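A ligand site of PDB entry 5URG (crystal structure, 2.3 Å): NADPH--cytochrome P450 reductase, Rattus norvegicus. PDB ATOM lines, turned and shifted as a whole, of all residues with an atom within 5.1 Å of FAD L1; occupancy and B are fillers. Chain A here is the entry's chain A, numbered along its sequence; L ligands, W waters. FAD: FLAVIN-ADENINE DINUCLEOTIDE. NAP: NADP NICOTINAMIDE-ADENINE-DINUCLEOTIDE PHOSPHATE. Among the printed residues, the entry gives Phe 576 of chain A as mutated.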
ATOM      1  N   HIS A 263      -7.139  -2.347 -24.527  1.00  0.00           N
ATOM      2  CA  HIS A 263      -7.094  -1.692 -23.231  1.00  0.00           C
ATOM      3  C   HIS A 263      -6.706  -2.717 -22.169  1.00  0.00           C
ATOM      4  O   HIS A 263      -7.011  -3.904 -22.303  1.00  0.00           O
ATOM      5  CB  HIS A 263      -8.457  -1.114 -22.862  1.00  0.00           C
ATOM      6  CG  HIS A 263      -8.984  -0.142 -23.862  1.00  0.00           C
ATOM      7  ND1 HIS A 263      -9.871  -0.504 -24.861  1.00  0.00           N
ATOM      8  CD2 HIS A 263      -8.704   1.165 -24.062  1.00  0.00           C
ATOM      9  CE1 HIS A 263     -10.108   0.542 -25.623  1.00  0.00           C
ATOM     10  NE2 HIS A 263      -9.416   1.571 -25.167  1.00  0.00           N
ATOM     11  N   THR A 322     -15.160   6.256  -2.632  1.00  0.00           N
ATOM     12  CA  THR A 322     -14.762   7.581  -3.101  1.00  0.00           C
ATOM     13  C   THR A 322     -15.786   8.351  -3.944  1.00  0.00           C
ATOM     14  O   THR A 322     -15.848   9.582  -3.858  1.00  0.00           O
ATOM     15  CB  THR A 322     -13.428   7.504  -3.865  1.00  0.00           C
ATOM     16  OG1 THR A 322     -13.563   6.629  -4.982  1.00  0.00           O
ATOM     17  CG2 THR A 322     -12.317   6.976  -2.950  1.00  0.00           C
ATOM     18  N   ASN A 323     -16.562   7.664  -4.765  1.00  0.00           N
ATOM     19  CA  ASN A 323     -17.554   8.375  -5.569  1.00  0.00           C
ATOM     20  C   ASN A 323     -18.746   8.772  -4.688  1.00  0.00           C
ATOM     21  O   ASN A 323     -19.018   8.118  -3.697  1.00  0.00           O
ATOM     22  CB  ASN A 323     -18.027   7.509  -6.747  1.00  0.00           C
ATOM     23  CG  ASN A 323     -16.933   7.287  -7.789  1.00  0.00           C
ATOM     24  OD1 ASN A 323     -16.259   8.239  -8.196  1.00  0.00           O
ATOM     25  ND2 ASN A 323     -16.771   6.042  -8.222  1.00  0.00           N
ATOM     26  N   ARG A 368     -18.617  16.415  -4.824  1.00  0.00           N
ATOM     27  CA  ARG A 368     -17.892  15.163  -4.866  1.00  0.00           C
ATOM     28  C   ARG A 368     -17.583  14.634  -3.467  1.00  0.00           C
ATOM     29  O   ARG A 368     -16.506  14.080  -3.220  1.00  0.00           O
ATOM     30  CB  ARG A 368     -16.588  15.367  -5.657  1.00  0.00           C
ATOM     31  CG  ARG A 368     -16.793  15.832  -7.100  1.00  0.00           C
ATOM     32  CD  ARG A 368     -17.236  14.692  -7.982  1.00  0.00           C
ATOM     33  NE  ARG A 368     -16.357  13.545  -7.767  1.00  0.00           N
ATOM     34  CZ  ARG A 368     -16.541  12.329  -8.303  1.00  0.00           C
ATOM     35  NH1 ARG A 368     -15.676  11.372  -8.022  1.00  0.00           N
ATOM     36  NH2 ARG A 368     -17.571  12.084  -9.100  1.00  0.00           N
ATOM     37  N   ARG A 398     -10.353  -0.172 -13.535  1.00  0.00           N
ATOM     38  CA  ARG A 398     -10.100   1.011 -14.332  1.00  0.00           C
ATOM     39  C   ARG A 398      -9.392   0.535 -15.602  1.00  0.00           C
ATOM     40  O   ARG A 398      -8.572  -0.391 -15.548  1.00  0.00           O
ATOM     41  CB  ARG A 398      -9.211   2.016 -13.583  1.00  0.00           C
ATOM     42  CG  ARG A 398      -9.965   3.040 -12.741  1.00  0.00           C
ATOM     43  CD  ARG A 398     -10.783   2.430 -11.611  1.00  0.00           C
ATOM     44  NE  ARG A 398     -11.390   3.483 -10.798  1.00  0.00           N
ATOM     45  CZ  ARG A 398     -12.127   3.294  -9.709  1.00  0.00           C
ATOM     46  NH1 ARG A 398     -12.614   4.339  -9.058  1.00  0.00           N
ATOM     47  NH2 ARG A 398     -12.368   2.064  -9.261  1.00  0.00           N
ATOM     48  N   TYR A 399      -9.717   1.176 -16.721  1.00  0.00           N
ATOM     49  CA  TYR A 399      -9.128   0.820 -18.014  1.00  0.00           C
ATOM     50  C   TYR A 399      -8.095   1.818 -18.498  1.00  0.00           C
ATOM     51  O   TYR A 399      -8.160   3.013 -18.203  1.00  0.00           O
ATOM     52  CB  TYR A 399     -10.229   0.667 -19.065  1.00  0.00           C
ATOM     53  CG  TYR A 399     -11.086  -0.554 -18.910  1.00  0.00           C
ATOM     54  CD1 TYR A 399     -12.118  -0.600 -17.971  1.00  0.00           C
ATOM     55  CD2 TYR A 399     -10.855  -1.687 -19.691  1.00  0.00           C
ATOM     56  CE1 TYR A 399     -12.885  -1.750 -17.795  1.00  0.00           C
ATOM     57  CE2 TYR A 399     -11.609  -2.845 -19.531  1.00  0.00           C
ATOM     58  CZ  TYR A 399     -12.628  -2.871 -18.587  1.00  0.00           C
ATOM     59  OH  TYR A 399     -13.364  -4.033 -18.423  1.00  0.00           O
ATOM     60  N   TYR A 400      -7.141   1.318 -19.282  1.00  0.00           N
ATOM     61  CA  TYR A 400      -6.071   2.145 -19.823  1.00  0.00           C
ATOM     62  C   TYR A 400      -5.684   1.646 -21.204  1.00  0.00           C
ATOM     63  O   TYR A 400      -5.643   0.443 -21.446  1.00  0.00           O
ATOM     64  CB  TYR A 400      -4.882   2.066 -18.874  1.00  0.00           C
ATOM     65  CG  TYR A 400      -5.196   2.658 -17.517  1.00  0.00           C
ATOM     66  CD1 TYR A 400      -5.156   4.033 -17.317  1.00  0.00           C
ATOM     67  CD2 TYR A 400      -5.603   1.841 -16.465  1.00  0.00           C
ATOM     68  CE1 TYR A 400      -5.523   4.601 -16.101  1.00  0.00           C
ATOM     69  CE2 TYR A 400      -5.976   2.407 -15.227  1.00  0.00           C
ATOM     70  CZ  TYR A 400      -5.927   3.790 -15.061  1.00  0.00           C
ATOM     71  OH  TYR A 400      -6.306   4.384 -13.869  1.00  0.00           O
ATOM     72  N   SER A 401      -5.423   2.563 -22.135  1.00  0.00           N
ATOM     73  CA  SER A 401      -5.034   2.170 -23.492  1.00  0.00           C
ATOM     74  C   SER A 401      -3.588   1.668 -23.452  1.00  0.00           C
ATOM     75  O   SER A 401      -2.666   2.443 -23.184  1.00  0.00           O
ATOM     76  CB  SER A 401      -5.139   3.355 -24.448  1.00  0.00           C
ATOM     77  OG  SER A 401      -6.443   3.878 -24.417  1.00  0.00           O
ATOM     78  N   CYS A 416       0.159   4.537 -19.705  1.00  0.00           N
ATOM     79  CA  CYS A 416       0.421   5.961 -19.703  1.00  0.00           C
ATOM     80  C   CYS A 416      -0.793   6.626 -19.071  1.00  0.00           C
ATOM     81  O   CYS A 416      -1.848   6.734 -19.684  1.00  0.00           O
ATOM     82  CB  CYS A 416       0.614   6.461 -21.136  1.00  0.00           C
ATOM     83  SG  CYS A 416       0.758   8.242 -21.260  1.00  0.00           S
ATOM     84  N   ALA A 417      -0.631   7.090 -17.833  1.00  0.00           N
ATOM     85  CA  ALA A 417      -1.742   7.684 -17.113  1.00  0.00           C
ATOM     86  C   ALA A 417      -1.439   8.975 -16.368  1.00  0.00           C
ATOM     87  O   ALA A 417      -0.305   9.189 -15.900  1.00  0.00           O
ATOM     88  CB  ALA A 417      -2.290   6.669 -16.138  1.00  0.00           C
ATOM     89  N   VAL A 418      -2.447   9.824 -16.250  1.00  0.00           N
ATOM     90  CA  VAL A 418      -2.298  11.067 -15.503  1.00  0.00           C
ATOM     91  C   VAL A 418      -2.885  10.824 -14.118  1.00  0.00           C
ATOM     92  O   VAL A 418      -4.030  10.380 -13.999  1.00  0.00           O
ATOM     93  CB  VAL A 418      -3.056  12.259 -16.160  1.00  0.00           C
ATOM     94  CG1 VAL A 418      -4.474  11.857 -16.528  1.00  0.00           C
ATOM     95  CG2 VAL A 418      -3.110  13.428 -15.179  1.00  0.00           C
ATOM     96  N   VAL A 420      -4.815  11.378 -10.837  1.00  0.00           N
ATOM     97  CA  VAL A 420      -5.920  12.259 -10.510  1.00  0.00           C
ATOM     98  C   VAL A 420      -5.807  12.717  -9.072  1.00  0.00           C
ATOM     99  O   VAL A 420      -5.550  11.919  -8.174  1.00  0.00           O
ATOM    100  CB  VAL A 420      -7.269  11.555 -10.726  1.00  0.00           C
ATOM    101  CG1 VAL A 420      -8.402  12.391 -10.136  1.00  0.00           C
ATOM    102  CG2 VAL A 420      -7.494  11.359 -12.209  1.00  0.00           C
ATOM    103  N   TYR A 422      -7.337  16.567  -7.103  1.00  0.00           N
ATOM    104  CA  TYR A 422      -7.972  17.851  -7.373  1.00  0.00           C
ATOM    105  C   TYR A 422      -8.647  18.340  -6.103  1.00  0.00           C
ATOM    106  O   TYR A 422      -8.813  17.593  -5.146  1.00  0.00           O
ATOM    107  CB  TYR A 422      -9.005  17.859  -8.508  1.00  0.00           C
ATOM    108  CG  TYR A 422     -10.129  16.871  -8.250  1.00  0.00           C
ATOM    109  CD1 TYR A 422      -9.939  15.505  -8.447  1.00  0.00           C
ATOM    110  CD2 TYR A 422     -11.370  17.299  -7.758  1.00  0.00           C
ATOM    111  CE1 TYR A 422     -10.957  14.579  -8.152  1.00  0.00           C
ATOM    112  CE2 TYR A 422     -12.388  16.373  -7.463  1.00  0.00           C
ATOM    113  CZ  TYR A 422     -12.178  15.016  -7.649  1.00  0.00           C
ATOM    114  OH  TYR A 422     -13.145  14.095  -7.304  1.00  0.00           O
ATOM    115  N   LYS A 431      -8.636  12.018  -4.251  1.00  0.00           N
ATOM    116  CA  LYS A 431      -7.605  11.252  -4.930  1.00  0.00           C
ATOM    117  C   LYS A 431      -8.227  10.169  -5.809  1.00  0.00           C
ATOM    118  O   LYS A 431      -9.199   9.512  -5.426  1.00  0.00           O
ATOM    119  CB  LYS A 431      -6.694  10.577  -3.893  1.00  0.00           C
ATOM    120  CG  LYS A 431      -5.980  11.549  -2.955  1.00  0.00           C
ATOM    121  CD  LYS A 431      -4.889  12.323  -3.667  1.00  0.00           C
ATOM    122  CE  LYS A 431      -3.677  11.450  -3.958  1.00  0.00           C
ATOM    123  NZ  LYS A 431      -2.990  11.034  -2.713  1.00  0.00           N
ATOM    124  N   GLY A 432      -7.670  10.005  -7.009  1.00  0.00           N
ATOM    125  CA  GLY A 432      -8.150   8.996  -7.947  1.00  0.00           C
ATOM    126  C   GLY A 432      -7.718   7.657  -7.386  1.00  0.00           C
ATOM    127  O   GLY A 432      -6.554   7.480  -7.021  1.00  0.00           O
ATOM    128  N   VAL A 433      -8.653   6.718  -7.321  1.00  0.00           N
ATOM    129  CA  VAL A 433      -8.351   5.411  -6.761  1.00  0.00           C
ATOM    130  C   VAL A 433      -7.232   4.649  -7.459  1.00  0.00           C
ATOM    131  O   VAL A 433      -6.200   4.341  -6.848  1.00  0.00           O
ATOM    132  CB  VAL A 433      -9.604   4.529  -6.762  1.00  0.00           C
ATOM    133  CG1 VAL A 433      -9.285   3.166  -6.134  1.00  0.00           C
ATOM    134  CG2 VAL A 433     -10.749   5.235  -5.993  1.00  0.00           C
ATOM    135  N   ALA A 434      -7.428   4.355  -8.736  1.00  0.00           N
ATOM    136  CA  ALA A 434      -6.459   3.596  -9.503  1.00  0.00           C
ATOM    137  C   ALA A 434      -5.148   4.326  -9.771  1.00  0.00           C
ATOM    138  O   ALA A 434      -4.073   3.716  -9.687  1.00  0.00           O
ATOM    139  CB  ALA A 434      -7.068   3.137 -10.830  1.00  0.00           C
ATOM    140  N   THR A 435      -5.199   5.625 -10.078  1.00  0.00           N
ATOM    141  CA  THR A 435      -3.964   6.331 -10.349  1.00  0.00           C
ATOM    142  C   THR A 435      -3.098   6.583  -9.115  1.00  0.00           C
ATOM    143  O   THR A 435      -1.876   6.590  -9.214  1.00  0.00           O
ATOM    144  CB  THR A 435      -4.198   7.633 -11.156  1.00  0.00           C
ATOM    145  OG1 THR A 435      -5.158   8.469 -10.503  1.00  0.00           O
ATOM    146  CG2 THR A 435      -4.677   7.279 -12.555  1.00  0.00           C
ATOM    147  N   SER A 436      -3.721   6.755  -7.941  1.00  0.00           N
ATOM    148  CA  SER A 436      -2.924   6.942  -6.727  1.00  0.00           C
ATOM    149  C   SER A 436      -2.233   5.601  -6.424  1.00  0.00           C
ATOM    150  O   SER A 436      -1.042   5.531  -6.140  1.00  0.00           O
ATOM    151  CB  SER A 436      -3.811   7.307  -5.531  1.00  0.00           C
ATOM    152  OG  SER A 436      -4.448   8.550  -5.732  1.00  0.00           O
ATOM    153  N   ARG A 458      -8.724  -6.271 -22.434  1.00  0.00           N
ATOM    154  CA  ARG A 458     -10.013  -6.163 -23.119  1.00  0.00           C
ATOM    155  C   ARG A 458      -9.719  -5.822 -24.560  1.00  0.00           C
ATOM    156  O   ARG A 458      -9.176  -4.757 -24.860  1.00  0.00           O
ATOM    157  CB  ARG A 458     -10.840  -5.048 -22.477  1.00  0.00           C
ATOM    158  CG  ARG A 458     -12.358  -5.195 -22.591  1.00  0.00           C
ATOM    159  CD  ARG A 458     -12.975  -4.136 -23.498  1.00  0.00           C
ATOM    160  NE  ARG A 458     -12.716  -2.739 -23.107  1.00  0.00           N
ATOM    161  CZ  ARG A 458     -13.398  -2.056 -22.196  1.00  0.00           C
ATOM    162  NH1 ARG A 458     -14.405  -2.598 -21.537  1.00  0.00           N
ATOM    163  NH2 ARG A 458     -13.074  -0.794 -21.958  1.00  0.00           N
ATOM    164  N   THR A 479      -2.672  12.958 -22.755  1.00  0.00           N
ATOM    165  CA  THR A 479      -2.574  11.549 -22.418  1.00  0.00           C
ATOM    166  C   THR A 479      -3.069  10.634 -23.537  1.00  0.00           C
ATOM    167  O   THR A 479      -2.770   9.449 -23.536  1.00  0.00           O
ATOM    168  CB  THR A 479      -3.360  11.262 -21.147  1.00  0.00           C
ATOM    169  OG1 THR A 479      -3.011  12.233 -20.162  1.00  0.00           O
ATOM    170  CG2 THR A 479      -3.040   9.884 -20.622  1.00  0.00           C
ATOM    171  N   ALA A 482      -1.194   7.751 -25.476  1.00  0.00           N
ATOM    172  CA  ALA A 482      -1.045   6.383 -25.016  1.00  0.00           C
ATOM    173  C   ALA A 482      -1.095   5.206 -26.001  1.00  0.00           C
ATOM    174  O   ALA A 482      -0.096   4.487 -26.160  1.00  0.00           O
ATOM    175  CB  ALA A 482      -2.097   6.095 -23.942  1.00  0.00           C
ATOM    176  N   PHE A 576      -9.214  12.174 -23.704  1.00  0.00           N
ATOM    177  CA  PHE A 576     -10.302  12.310 -22.747  1.00  0.00           C
ATOM    178  C   PHE A 576     -11.499  13.098 -23.289  1.00  0.00           C
ATOM    179  O   PHE A 576     -12.603  12.568 -23.358  1.00  0.00           O
ATOM    180  CB  PHE A 576      -9.812  13.026 -21.486  1.00  0.00           C
ATOM    181  CG  PHE A 576      -9.125  12.116 -20.505  1.00  0.00           C
ATOM    182  CD1 PHE A 576      -9.852  11.210 -19.755  1.00  0.00           C
ATOM    183  CD2 PHE A 576      -7.733  12.148 -20.378  1.00  0.00           C
ATOM    184  CE1 PHE A 576      -9.206  10.338 -18.882  1.00  0.00           C
ATOM    185  CE2 PHE A 576      -7.085  11.285 -19.509  1.00  0.00           C
ATOM    186  CZ  PHE A 576      -7.802  10.377 -18.756  1.00  0.00           C
ATOM    187  N   ASP A 619     -11.070   6.381 -29.752  1.00  0.00           N
ATOM    188  CA  ASP A 619     -10.865   5.808 -28.429  1.00  0.00           C
ATOM    189  C   ASP A 619     -10.911   7.010 -27.503  1.00  0.00           C
ATOM    190  O   ASP A 619      -9.866   7.497 -27.037  1.00  0.00           O
ATOM    191  CB  ASP A 619      -9.521   5.106 -28.319  1.00  0.00           C
ATOM    192  CG  ASP A 619      -9.310   4.453 -26.943  1.00  0.00           C
ATOM    193  OD1 ASP A 619     -10.300   3.982 -26.352  1.00  0.00           O
ATOM    194  OD2 ASP A 619      -8.159   4.401 -26.477  1.00  0.00           O
ATOM    195  N   TRP A 621     -12.156   8.601 -23.999  1.00  0.00           N
ATOM    196  CA  TRP A 621     -12.412   8.111 -22.646  1.00  0.00           C
ATOM    197  C   TRP A 621     -13.481   8.811 -21.808  1.00  0.00           C
ATOM    198  O   TRP A 621     -13.575   8.591 -20.597  1.00  0.00           O
ATOM    199  CB  TRP A 621     -11.094   8.111 -21.879  1.00  0.00           C
ATOM    200  CG  TRP A 621      -9.982   7.510 -22.651  1.00  0.00           C
ATOM    201  CD1 TRP A 621     -10.072   6.534 -23.590  1.00  0.00           C
ATOM    202  CD2 TRP A 621      -8.594   7.825 -22.526  1.00  0.00           C
ATOM    203  NE1 TRP A 621      -8.828   6.208 -24.067  1.00  0.00           N
ATOM    204  CE2 TRP A 621      -7.900   6.980 -23.427  1.00  0.00           C
ATOM    205  CE3 TRP A 621      -7.866   8.729 -21.744  1.00  0.00           C
ATOM    206  CZ2 TRP A 621      -6.519   7.023 -23.556  1.00  0.00           C
ATOM    207  CZ3 TRP A 621      -6.496   8.764 -21.872  1.00  0.00           C
ATOM    208  CH2 TRP A 621      -5.833   7.915 -22.776  1.00  0.00           C
HETATM  209  PA  FAD L   1     -11.346   7.759  -9.944  1.00  0.00           P
HETATM  210  O1A FAD L   1     -11.327   7.509  -8.485  1.00  0.00           O
HETATM  211  O2A FAD L   1     -11.976   6.754 -10.823  1.00  0.00           O
HETATM  212  O5B FAD L   1     -12.023   9.192 -10.193  1.00  0.00           O
HETATM  213  C5B FAD L   1     -12.405   9.593 -11.510  1.00  0.00           C
HETATM  214  C4B FAD L   1     -13.497  10.664 -11.407  1.00  0.00           C
HETATM  215  O4B FAD L   1     -13.053  11.777 -10.634  1.00  0.00           O
HETATM  216  C3B FAD L   1     -13.792  11.281 -12.761  1.00  0.00           C
HETATM  217  O3B FAD L   1     -14.651  10.404 -13.501  1.00  0.00           O
HETATM  218  C2B FAD L   1     -14.622  12.463 -12.276  1.00  0.00           C
HETATM  219  O2B FAD L   1     -15.940  12.025 -11.950  1.00  0.00           O
HETATM  220  C1B FAD L   1     -13.867  12.892 -11.021  1.00  0.00           C
HETATM  221  N9A FAD L   1     -12.915  13.989 -11.308  1.00  0.00           N
HETATM  222  C8A FAD L   1     -11.588  13.834 -11.924  1.00  0.00           C
HETATM  223  N7A FAD L   1     -11.078  15.211 -11.818  1.00  0.00           N
HETATM  224  C5A FAD L   1     -12.046  15.999 -11.344  1.00  0.00           C
HETATM  225  C6A FAD L   1     -12.020  17.297 -11.095  1.00  0.00           C
HETATM  226  N6A FAD L   1     -10.835  17.900 -11.225  1.00  0.00           N
HETATM  227  N1A FAD L   1     -13.062  17.957 -10.573  1.00  0.00           N
HETATM  228  C2A FAD L   1     -14.232  17.243 -10.277  1.00  0.00           C
HETATM  229  N3A FAD L   1     -14.224  15.862 -10.553  1.00  0.00           N
HETATM  230  C4A FAD L   1     -13.137  15.278 -11.076  1.00  0.00           C
HETATM  231  N1  FAD L   1      -6.651   7.427 -18.337  1.00  0.00           N
HETATM  232  C2  FAD L   1      -5.281   7.626 -18.529  1.00  0.00           C
HETATM  233  O2  FAD L   1      -4.682   8.493 -17.884  1.00  0.00           O
HETATM  234  N3  FAD L   1      -4.611   6.887 -19.518  1.00  0.00           N
HETATM  235  C4  FAD L   1      -5.313   5.956 -20.297  1.00  0.00           C
HETATM  236  O4  FAD L   1      -4.690   5.215 -21.043  1.00  0.00           O
HETATM  237  C4X FAD L   1      -6.691   5.807 -20.125  1.00  0.00           C
HETATM  238  N5  FAD L   1      -7.404   5.127 -21.036  1.00  0.00           N
HETATM  239  C5X FAD L   1      -8.724   4.968 -20.851  1.00  0.00           C
HETATM  240  C6  FAD L   1      -9.434   4.131 -21.711  1.00  0.00           C
HETATM  241  C7  FAD L   1     -10.765   3.827 -21.450  1.00  0.00           C
HETATM  242  C7M FAD L   1     -11.428   2.886 -22.229  1.00  0.00           C
HETATM  243  C8  FAD L   1     -11.392   4.380 -20.338  1.00  0.00           C
HETATM  244  C8M FAD L   1     -12.706   4.038 -20.048  1.00  0.00           C
HETATM  245  C9  FAD L   1     -10.679   5.223 -19.490  1.00  0.00           C
HETATM  246  C9A FAD L   1      -9.346   5.501 -19.730  1.00  0.00           C
HETATM  247  N10 FAD L   1      -8.615   6.204 -18.836  1.00  0.00           N
HETATM  248  C10 FAD L   1      -7.359   6.539 -19.155  1.00  0.00           C
HETATM  249  C1' FAD L   1      -9.234   6.769 -17.619  1.00  0.00           C
HETATM  250  C2' FAD L   1      -9.154   5.722 -16.503  1.00  0.00           C
HETATM  251  O2' FAD L   1      -9.941   4.592 -16.849  1.00  0.00           O
HETATM  252  C3' FAD L   1      -9.628   6.274 -15.157  1.00  0.00           C
HETATM  253  O3' FAD L   1     -10.954   6.790 -15.258  1.00  0.00           O
HETATM  254  C4' FAD L   1      -8.673   7.366 -14.670  1.00  0.00           C
HETATM  255  O4' FAD L   1      -7.337   6.842 -14.619  1.00  0.00           O
HETATM  256  C5' FAD L   1      -9.100   7.824 -13.281  1.00  0.00           C
HETATM  257  O5' FAD L   1      -9.245   6.674 -12.434  1.00  0.00           O
HETATM  258  P   FAD L   1      -8.907   6.742 -10.861  1.00  0.00           P
HETATM  259  O1P FAD L   1      -9.515   5.561 -10.190  1.00  0.00           O
HETATM  260  O2P FAD L   1      -7.509   7.153 -10.576  1.00  0.00           O
HETATM  261  O3P FAD L   1      -9.829   7.980 -10.434  1.00  0.00           O
HETATM  262  PA  NAP L   2      -4.435  18.217 -20.906  1.00  0.00           P
HETATM  263  O1A NAP L   2      -3.184  18.970 -20.682  1.00  0.00           O
HETATM  264  O2A NAP L   2      -5.727  18.841 -20.543  1.00  0.00           O
HETATM  265  O5B NAP L   2      -4.462  17.717 -22.433  1.00  0.00           O
HETATM  266  C5B NAP L   2      -5.226  18.390 -23.432  1.00  0.00           C
HETATM  267  C4B NAP L   2      -4.240  19.018 -24.422  1.00  0.00           C
HETATM  268  O4B NAP L   2      -4.979  19.418 -25.594  1.00  0.00           O
HETATM  269  C3B NAP L   2      -3.707  20.322 -23.849  1.00  0.00           C
HETATM  270  O3B NAP L   2      -2.599  20.796 -24.628  1.00  0.00           O
HETATM  271  C2B NAP L   2      -4.937  21.196 -24.007  1.00  0.00           C
HETATM  272  O2B NAP L   2      -4.542  22.575 -24.074  1.00  0.00           O
HETATM  273  C1B NAP L   2      -5.402  20.770 -25.387  1.00  0.00           C
HETATM  274  N9A NAP L   2      -6.858  20.922 -25.596  1.00  0.00           N
HETATM  275  C8A NAP L   2      -7.755  21.359 -24.702  1.00  0.00           C
HETATM  276  N7A NAP L   2      -8.928  21.438 -25.324  1.00  0.00           N
HETATM  277  C5A NAP L   2      -8.768  21.060 -26.583  1.00  0.00           C
HETATM  278  C6A NAP L   2      -9.630  20.960 -27.593  1.00  0.00           C
HETATM  279  N6A NAP L   2     -10.868  21.403 -27.367  1.00  0.00           N
HETATM  280  N1A NAP L   2      -9.273  20.478 -28.789  1.00  0.00           N
HETATM  281  C2A NAP L   2      -7.941  20.076 -28.983  1.00  0.00           C
HETATM  282  N3A NAP L   2      -7.055  20.224 -27.912  1.00  0.00           N
HETATM  283  C4A NAP L   2      -7.497  20.717 -26.744  1.00  0.00           C
HETATM  284  O3  NAP L   2      -4.323  16.797 -20.150  1.00  0.00           O
HETATM  285  PN  NAP L   2      -5.029  15.403 -20.543  1.00  0.00           P
HETATM  286  O1N NAP L   2      -4.599  14.367 -19.578  1.00  0.00           O
HETATM  287  O2N NAP L   2      -4.826  15.147 -21.984  1.00  0.00           O
HETATM  288  O5D NAP L   2      -6.590  15.735 -20.308  1.00  0.00           O
HETATM  289  C5D NAP L   2      -7.291  16.509 -21.282  1.00  0.00           C
HETATM  290  C4D NAP L   2      -8.699  16.882 -20.786  1.00  0.00           C
HETATM  291  O4D NAP L   2      -9.484  15.741 -20.443  1.00  0.00           O
HETATM  292  C3D NAP L   2      -8.653  17.729 -19.533  1.00  0.00           C
HETATM  293  O3D NAP L   2      -8.367  19.088 -19.860  1.00  0.00           O
HETATM  294  C2D NAP L   2     -10.124  17.617 -19.164  1.00  0.00           C
HETATM  295  O2D NAP L   2     -10.935  18.301 -20.133  1.00  0.00           O
HETATM  296  C1D NAP L   2     -10.317  16.118 -19.331  1.00  0.00           C
HETATM  297  N1N NAP L   2      -9.849  15.380 -18.138  1.00  0.00           N
HETATM  298  C2N NAP L   2     -10.747  15.067 -17.116  1.00  0.00           C
HETATM  299  C3N NAP L   2     -10.385  14.169 -16.118  1.00  0.00           C
HETATM  300  C4N NAP L   2      -9.094  13.645 -16.097  1.00  0.00           C
HETATM  301  C5N NAP L   2      -8.177  13.983 -17.094  1.00  0.00           C
HETATM  302  C6N NAP L   2      -8.549  14.842 -18.121  1.00  0.00           C
HETATM  303  P2B NAP L   2      -5.022  23.661 -22.981  1.00  0.00           P
HETATM  304  O1X NAP L   2      -6.319  24.131 -23.504  1.00  0.00           O
HETATM  305  O2X NAP L   2      -3.935  24.667 -23.025  1.00  0.00           O
HETATM  306  O3X NAP L   2      -5.095  22.898 -21.719  1.00  0.00           O
HETATM  307  O   HOH W   1      -2.255   3.929 -20.856  1.00  0.00           O
HETATM  308  O   HOH W   2     -12.712  11.255  -7.560  1.00  0.00           O
HETATM  309  O   HOH W   3     -11.664   9.296 -15.788  1.00  0.00           O
HETATM  310  O   HOH W   4     -13.942   7.378  -7.337  1.00  0.00           O
HETATM  311  O   HOH W   5      -5.991   9.093 -15.527  1.00  0.00           O
HETATM  312  O   HOH W   6     -11.981   2.913 -16.424  1.00  0.00           O
HETATM  313  O   HOH W   7     -12.345   6.204 -13.181  1.00  0.00           O
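N of Thr 435 sits at hydrogen-bond distance from O2P of FAD L1, 2.8 Å away. An oxygen (O2P) of FAD L1 is in hydrogen-bond range of the side-chain hydroxyl of Thr 435 (2.7 Å). N of Tyr 399 sits at hydrogen-bond distance from O2' of FAD L1 (3.4 Å). The backbone carbonyl oxygen (O) of Tyr 399 is in hydrogen-bond range of an oxygen (O2') of FAD L1, at 2.7 Å. The side-chain hydroxyl (OH) of Tyr 400 is in hydrogen-bond range of an oxygen (O4') of FAD L1, at 2.8 Å. The backbone carbonyl oxygen (O) of Cys 416 is in hydrogen-bond range of a nitrogen (N3) of FAD L1 (2.8 Å). O1P of FAD L1 sits at hydrogen-bond distance from N of Ala 434, at 2.8 Å. NE of Arg 398 is in salt-bridge range of O1P of FAD L1, 2.9 Å away. The backbone NH of Ser 401 sits at hydrogen-bond distance from an oxygen (O4) of FAD L1, 3.0 Å away. An oxygen (O1A) of FAD L1 is in hydrogen-bond range of the backbone NH (N) of Val 433, 3.0 Å away. The backbone NH (N) of Val 418 is in hydrogen-bond range of an oxygen (O2) of FAD L1 (3.1 Å). The guanidinium group of Arg 368 sits at hydrogen-bond distance from an oxygen (O2B) of FAD L1. N of Thr 479 lies within hydrogen-bond range of O2N of NAP L2. An oxygen (O1N) of NAP L2 lies within hydrogen-bond range of the side-chain hydroxyl (OG1) of Thr 479 (2.7 Å).
The side-chain hydroxyl (OG1) of Thr 435 is in hydrogen-bond range of the backbone NH (N) of Val 420, 2.9 Å away. OG of Ser 401 lies close to NE1 of Trp 621. The side-chain hydroxyl (OG) of Ser 401 sits at hydrogen-bond distance from the side-chain carboxylate (OD2) of Asp 619 (2.7 Å). The side-chain carboxylate of Asp 619 lies within hydrogen-bond range of the indole nitrogen of Trp 621, at 3.1 Å. N of Gly 432 is in hydrogen-bond range of O of Val 420 (3.1 Å). The backbone carbonyl oxygen (O) of Gly 432 lies within hydrogen-bond range of the side-chain hydroxyl (OG) of Ser 436 (2.7 Å). NH1 of Arg 368 is in hydrogen-bond range of OD1 of Asn 323. O of His 263 is in hydrogen-bond range of N of Arg 458 (2.9 Å).
His 263 touches FAD L1 (CD2 to C7M, 3.7 Å). Ala 417 touches FAD L1. CG1 of Val 420 touches C8A of FAD L1, 3.9 Å away. Tyr 422 touches FAD L1. CA of Gly 432 touches O3P of FAD L1, at 3.2 Å. Thr 479 touches FAD L1. Ala 482 touches FAD L1. Phe 576 touches FAD L1 (CZ to N1, 3.2 Å). CE2 of Trp 621 touches N5 of FAD L1 (3.1 Å). Hydrophobic or aromatic side chains that line FAD L1: His 263, Tyr 399, Tyr 400, Ala 417, Val 418, Val 420, Tyr 422, Val 433, Ala 434, Ala 482, Phe 576 and Trp 621. Of the 25 residues printed, 19 come within 4 Å of FAD L1. The nearest printed residue that does not touch FAD L1 is Arg 458 (4.04 Å).
Water W6 bridges O2' of FAD L1 and N of Tyr 399. Water W1 lies within hydrogen-bond range of N of Cys 416 (2.7 Å), O4 of FAD L1 (2.8 Å) and O of Ser 401 (2.8 Å). Water W5 bridges O2 of FAD L1 and O of Val 418. Water W4 lies within hydrogen-bond range of the side-chain hydroxyl of Thr 322, the side-chain amide oxygen of Asn 323 and an oxygen (O1A) of FAD L1. Water W2 lies within hydrogen-bond range of OH of Tyr 422 (2.9 Å), NH1 of Arg 368 (3.0 Å) and O4B of FAD L1 (3.1 Å).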
